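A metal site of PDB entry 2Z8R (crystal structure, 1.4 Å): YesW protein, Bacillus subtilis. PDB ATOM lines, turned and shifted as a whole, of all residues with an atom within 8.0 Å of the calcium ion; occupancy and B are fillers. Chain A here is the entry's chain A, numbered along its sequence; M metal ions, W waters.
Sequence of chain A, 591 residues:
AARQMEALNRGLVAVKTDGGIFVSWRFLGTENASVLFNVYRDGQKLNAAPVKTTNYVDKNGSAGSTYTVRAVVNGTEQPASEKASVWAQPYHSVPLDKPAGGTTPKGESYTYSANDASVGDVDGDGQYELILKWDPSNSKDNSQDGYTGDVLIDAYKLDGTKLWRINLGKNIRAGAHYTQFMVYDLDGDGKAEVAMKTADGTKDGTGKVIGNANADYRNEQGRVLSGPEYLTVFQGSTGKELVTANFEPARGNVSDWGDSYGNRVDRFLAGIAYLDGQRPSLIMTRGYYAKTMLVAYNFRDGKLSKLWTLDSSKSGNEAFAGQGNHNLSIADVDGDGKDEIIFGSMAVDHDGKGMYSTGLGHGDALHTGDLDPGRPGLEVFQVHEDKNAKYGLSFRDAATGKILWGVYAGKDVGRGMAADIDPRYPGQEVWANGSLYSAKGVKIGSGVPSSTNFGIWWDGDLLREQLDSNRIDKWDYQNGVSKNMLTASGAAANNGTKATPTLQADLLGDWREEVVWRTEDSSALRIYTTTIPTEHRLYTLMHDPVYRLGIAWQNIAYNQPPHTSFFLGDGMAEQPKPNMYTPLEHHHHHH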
ATOM      1  N   ASN A   9      -3.257 -19.321 -20.948  1.00  0.00           N
ATOM      2  CA  ASN A   9      -4.119 -18.428 -20.188  1.00  0.00           C
ATOM      3  C   ASN A   9      -5.514 -18.420 -20.836  1.00  0.00           C
ATOM      4  O   ASN A   9      -5.791 -19.256 -21.705  1.00  0.00           O
ATOM      5  CB  ASN A   9      -3.485 -17.023 -20.022  1.00  0.00           C
ATOM      6  CG  ASN A   9      -3.466 -16.206 -21.301  1.00  0.00           C
ATOM      7  OD1 ASN A   9      -4.034 -16.588 -22.327  1.00  0.00           O
ATOM      8  ND2 ASN A   9      -2.819 -15.029 -21.240  1.00  0.00           N
ATOM      9  N   GLY A 120       5.013 -20.036 -30.135  1.00  0.00           N
ATOM     10  CA  GLY A 120       5.336 -20.782 -28.930  1.00  0.00           C
ATOM     11  C   GLY A 120       5.239 -19.804 -27.774  1.00  0.00           C
ATOM     12  O   GLY A 120       5.338 -18.607 -27.970  1.00  0.00           O
ATOM     13  N   ASP A 121       5.063 -20.338 -26.575  1.00  0.00           N
ATOM     14  CA  ASP A 121       5.049 -19.503 -25.390  1.00  0.00           C
ATOM     15  C   ASP A 121       6.448 -19.596 -24.779  1.00  0.00           C
ATOM     16  O   ASP A 121       6.769 -20.560 -24.082  1.00  0.00           O
ATOM     17  CB  ASP A 121       3.980 -20.004 -24.410  1.00  0.00           C
ATOM     18  CG  ASP A 121       3.914 -19.188 -23.135  1.00  0.00           C
ATOM     19  OD1 ASP A 121       4.488 -18.083 -23.104  1.00  0.00           O
ATOM     20  OD2 ASP A 121       3.287 -19.660 -22.174  1.00  0.00           O
ATOM     21  N   VAL A 122       7.286 -18.609 -25.093  1.00  0.00           N
ATOM     22  CA  VAL A 122       8.701 -18.693 -24.729  1.00  0.00           C
ATOM     23  C   VAL A 122       8.978 -18.325 -23.269  1.00  0.00           C
ATOM     24  O   VAL A 122      10.039 -18.674 -22.736  1.00  0.00           O
ATOM     25  CB  VAL A 122       9.597 -17.838 -25.670  1.00  0.00           C
ATOM     26  CG1 VAL A 122       9.353 -18.210 -27.130  1.00  0.00           C
ATOM     27  CG2 VAL A 122       9.402 -16.332 -25.422  1.00  0.00           C
ATOM     28  N   ASP A 123       8.036 -17.647 -22.632  1.00  0.00           N
ATOM     29  CA  ASP A 123       8.227 -17.220 -21.244  1.00  0.00           C
ATOM     30  C   ASP A 123       7.255 -17.867 -20.249  1.00  0.00           C
ATOM     31  O   ASP A 123       7.362 -17.635 -19.048  1.00  0.00           O
ATOM     32  CB  ASP A 123       8.249 -15.680 -21.107  1.00  0.00           C
ATOM     33  CG  ASP A 123       6.996 -15.010 -21.627  1.00  0.00           C
ATOM     34  OD1 ASP A 123       6.135 -15.679 -22.243  1.00  0.00           O
ATOM     35  OD2 ASP A 123       6.881 -13.778 -21.440  1.00  0.00           O
ATOM     36  N   GLY A 124       6.317 -18.680 -20.749  1.00  0.00           N
ATOM     37  CA  GLY A 124       5.499 -19.519 -19.878  1.00  0.00           C
ATOM     38  C   GLY A 124       4.298 -18.855 -19.218  1.00  0.00           C
ATOM     39  O   GLY A 124       3.754 -19.389 -18.250  1.00  0.00           O
ATOM     40  N   ASP A 125       3.859 -17.720 -19.758  1.00  0.00           N
ATOM     41  CA  ASP A 125       2.705 -17.013 -19.179  1.00  0.00           C
ATOM     42  C   ASP A 125       1.362 -17.399 -19.809  1.00  0.00           C
ATOM     43  O   ASP A 125       0.312 -16.873 -19.432  1.00  0.00           O
ATOM     44  CB  ASP A 125       2.902 -15.489 -19.238  1.00  0.00           C
ATOM     45  CG  ASP A 125       2.851 -14.945 -20.656  1.00  0.00           C
ATOM     46  OD1 ASP A 125       2.955 -15.724 -21.637  1.00  0.00           O
ATOM     47  OD2 ASP A 125       2.709 -13.707 -20.802  1.00  0.00           O
ATOM     48  N   GLY A 126       1.387 -18.321 -20.768  1.00  0.00           N
ATOM     49  CA  GLY A 126       0.139 -18.786 -21.387  1.00  0.00           C
ATOM     50  C   GLY A 126      -0.365 -17.969 -22.567  1.00  0.00           C
ATOM     51  O   GLY A 126      -1.449 -18.233 -23.088  1.00  0.00           O
ATOM     52  N   GLN A 127       0.424 -16.981 -22.980  1.00  0.00           N
ATOM     53  CA  GLN A 127       0.170 -16.199 -24.196  1.00  0.00           C
ATOM     54  C   GLN A 127       1.264 -16.504 -25.216  1.00  0.00           C
ATOM     55  O   GLN A 127       2.450 -16.478 -24.876  1.00  0.00           O
ATOM     56  CB  GLN A 127       0.153 -14.707 -23.871  1.00  0.00           C
ATOM     57  CG  GLN A 127      -0.106 -13.845 -25.091  1.00  0.00           C
ATOM     58  CD  GLN A 127      -0.117 -12.376 -24.784  1.00  0.00           C
ATOM     59  OE1 GLN A 127      -1.114 -11.842 -24.307  1.00  0.00           O
ATOM     60  NE2 GLN A 127       0.994 -11.696 -25.085  1.00  0.00           N
ATOM     61  N   TYR A 128       0.892 -16.785 -26.467  1.00  0.00           N
ATOM     62  CA  TYR A 128       1.886 -17.109 -27.498  1.00  0.00           C
ATOM     63  C   TYR A 128       2.701 -15.898 -27.930  1.00  0.00           C
ATOM     64  O   TYR A 128       2.160 -14.783 -28.082  1.00  0.00           O
ATOM     65  CB  TYR A 128       1.200 -17.699 -28.733  1.00  0.00           C
ATOM     66  CG  TYR A 128       0.651 -19.078 -28.516  1.00  0.00           C
ATOM     67  CD1 TYR A 128       1.516 -20.157 -28.262  1.00  0.00           C
ATOM     68  CD2 TYR A 128      -0.723 -19.328 -28.562  1.00  0.00           C
ATOM     69  CE1 TYR A 128       1.021 -21.427 -28.042  1.00  0.00           C
ATOM     70  CE2 TYR A 128      -1.222 -20.607 -28.343  1.00  0.00           C
ATOM     71  CZ  TYR A 128      -0.340 -21.650 -28.085  1.00  0.00           C
ATOM     72  OH  TYR A 128      -0.841 -22.904 -27.889  1.00  0.00           O
ATOM     73  N   GLU A 129       3.994 -16.145 -28.155  1.00  0.00           N
ATOM     74  CA  GLU A 129       4.847 -15.254 -28.943  1.00  0.00           C
ATOM     75  C   GLU A 129       4.820 -15.705 -30.405  1.00  0.00           C
ATOM     76  O   GLU A 129       4.538 -16.884 -30.688  1.00  0.00           O
ATOM     77  CB  GLU A 129       6.291 -15.324 -28.434  1.00  0.00           C
ATOM     78  CG  GLU A 129       6.547 -14.515 -27.153  1.00  0.00           C
ATOM     79  CD  GLU A 129       5.734 -15.016 -25.956  1.00  0.00           C
ATOM     80  OE1 GLU A 129       5.879 -16.188 -25.538  1.00  0.00           O
ATOM     81  OE2 GLU A 129       4.973 -14.192 -25.392  1.00  0.00           O
ATOM     82  N   LEU A 130       5.113 -14.772 -31.308  1.00  0.00           N
ATOM     83  CA  LEU A 130       5.265 -15.068 -32.719  1.00  0.00           C
ATOM     84  C   LEU A 130       6.742 -15.211 -33.058  1.00  0.00           C
ATOM     85  O   LEU A 130       7.546 -14.340 -32.706  1.00  0.00           O
ATOM     86  CB  LEU A 130       4.646 -13.958 -33.567  1.00  0.00           C
ATOM     87  CG  LEU A 130       3.124 -13.994 -33.614  1.00  0.00           C
ATOM     88  CD1 LEU A 130       2.541 -12.616 -33.945  1.00  0.00           C
ATOM     89  CD2 LEU A 130       2.624 -15.045 -34.598  1.00  0.00           C
ATOM     90  N   TYR A 156       8.731 -12.107 -31.377  1.00  0.00           N
ATOM     91  CA  TYR A 156       7.959 -10.941 -30.932  1.00  0.00           C
ATOM     92  C   TYR A 156       6.901 -11.339 -29.931  1.00  0.00           C
ATOM     93  O   TYR A 156       6.194 -12.328 -30.122  1.00  0.00           O
ATOM     94  CB  TYR A 156       7.245 -10.281 -32.111  1.00  0.00           C
ATOM     95  CG  TYR A 156       8.180  -9.620 -33.075  1.00  0.00           C
ATOM     96  CD1 TYR A 156       8.585  -8.296 -32.906  1.00  0.00           C
ATOM     97  CD2 TYR A 156       8.667 -10.330 -34.190  1.00  0.00           C
ATOM     98  CE1 TYR A 156       9.466  -7.695 -33.802  1.00  0.00           C
ATOM     99  CE2 TYR A 156       9.544  -9.737 -35.086  1.00  0.00           C
ATOM    100  CZ  TYR A 156       9.939  -8.423 -34.899  1.00  0.00           C
ATOM    101  OH  TYR A 156      10.813  -7.853 -35.785  1.00  0.00           O
ATOM    102  N   LYS A 157       6.769 -10.544 -28.876  1.00  0.00           N
ATOM    103  CA  LYS A 157       5.568 -10.611 -28.034  1.00  0.00           C
ATOM    104  C   LYS A 157       4.429  -9.926 -28.770  1.00  0.00           C
ATOM    105  O   LYS A 157       4.664  -9.109 -29.677  1.00  0.00           O
ATOM    106  CB  LYS A 157       5.811  -9.948 -26.689  1.00  0.00           C
ATOM    107  CG  LYS A 157       6.849 -10.689 -25.836  1.00  0.00           C
ATOM    108  CD  LYS A 157       6.911 -10.127 -24.419  1.00  0.00           C
ATOM    109  CE  LYS A 157       5.798 -10.685 -23.534  1.00  0.00           C
ATOM    110  NZ  LYS A 157       6.045 -12.121 -23.160  1.00  0.00           N
ATOM    111  N   LEU A 158       3.200 -10.237 -28.392  1.00  0.00           N
ATOM    112  CA  LEU A 158       2.068  -9.657 -29.101  1.00  0.00           C
ATOM    113  C   LEU A 158       1.979  -8.132 -28.968  1.00  0.00           C
ATOM    114  O   LEU A 158       1.409  -7.465 -29.828  1.00  0.00           O
ATOM    115  CB  LEU A 158       0.748 -10.336 -28.729  1.00  0.00           C
ATOM    116  CG  LEU A 158       0.649 -11.852 -28.954  1.00  0.00           C
ATOM    117  CD1 LEU A 158      -0.785 -12.330 -28.708  1.00  0.00           C
ATOM    118  CD2 LEU A 158       1.140 -12.276 -30.349  1.00  0.00           C
ATOM    119  N   LEU A 163      11.997  -9.697 -28.968  1.00  0.00           N
ATOM    120  CA  LEU A 163      12.819 -10.395 -27.996  1.00  0.00           C
ATOM    121  C   LEU A 163      14.230 -10.690 -28.477  1.00  0.00           C
ATOM    122  O   LEU A 163      15.174 -10.636 -27.678  1.00  0.00           O
ATOM    123  CB  LEU A 163      12.148 -11.689 -27.527  1.00  0.00           C
ATOM    124  CG  LEU A 163      10.762 -11.523 -26.898  1.00  0.00           C
ATOM    125  CD1 LEU A 163      10.173 -12.862 -26.569  1.00  0.00           C
ATOM    126  CD2 LEU A 163      10.835 -10.671 -25.633  1.00  0.00           C
ATOM    127  N   GLY A 190       7.661 -25.836 -19.629  1.00  0.00           N
ATOM    128  CA  GLY A 190       6.630 -24.813 -19.786  1.00  0.00           C
ATOM    129  C   GLY A 190       6.987 -23.661 -20.727  1.00  0.00           C
ATOM    130  O   GLY A 190       6.173 -22.774 -20.969  1.00  0.00           O
HETATM  131 CA    CA M   1       4.285 -15.729 -23.620  1.00  0.00          CA
HETATM  132  O   HOH W   1       3.436 -13.415 -23.194  1.00  0.00           O
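The side-chain carboxylate (OD2) of Asp 123 is in salt-bridge range of the side-chain amino group (NZ) of Lys 157 (2.5 Å). The side-chain carboxylate (OE1) of Glu 129 lies close to the backbone NH (N) of Val 122 (2.8 Å). The backbone NH of Gly 124 sits close to the side-chain carboxylate of Asp 121, at 3.5 Å. N of Glu 129 sits at hydrogen-bond distance from O of Gly 120. OD2 of Asp 121 is in hydrogen-bond range of N of Gly 126 (2.7 Å). NZ of Lys 157 lies close to OE2 of Glu 129.
Water W1 lies within hydrogen-bond range of the side-chain carboxylate (OD2) of Asp 125 (2.5 Å) and the side-chain amino group (NZ) of Lys 157 (2.9 Å).
The calcium ion is bound by the side-chain carboxylate (OD1) of Asp 123, at 2.3 Å. O of Gln 127 binds the calcium ion, 2.3 Å away. OD1 of Asp 125 binds the calcium ion, at 2.4 Å. The calcium ion is bound by OD1 of Asp 121, 2.4 Å away. The side-chain carboxylate (OE2) of Glu 129 binds the calcium ion, 2.4 Å away. Water W1 is bound to the calcium ion (2.5 Å). The calcium ion is bound by the side-chain carboxylate (OE1) of Glu 129, 2.5 Å away.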
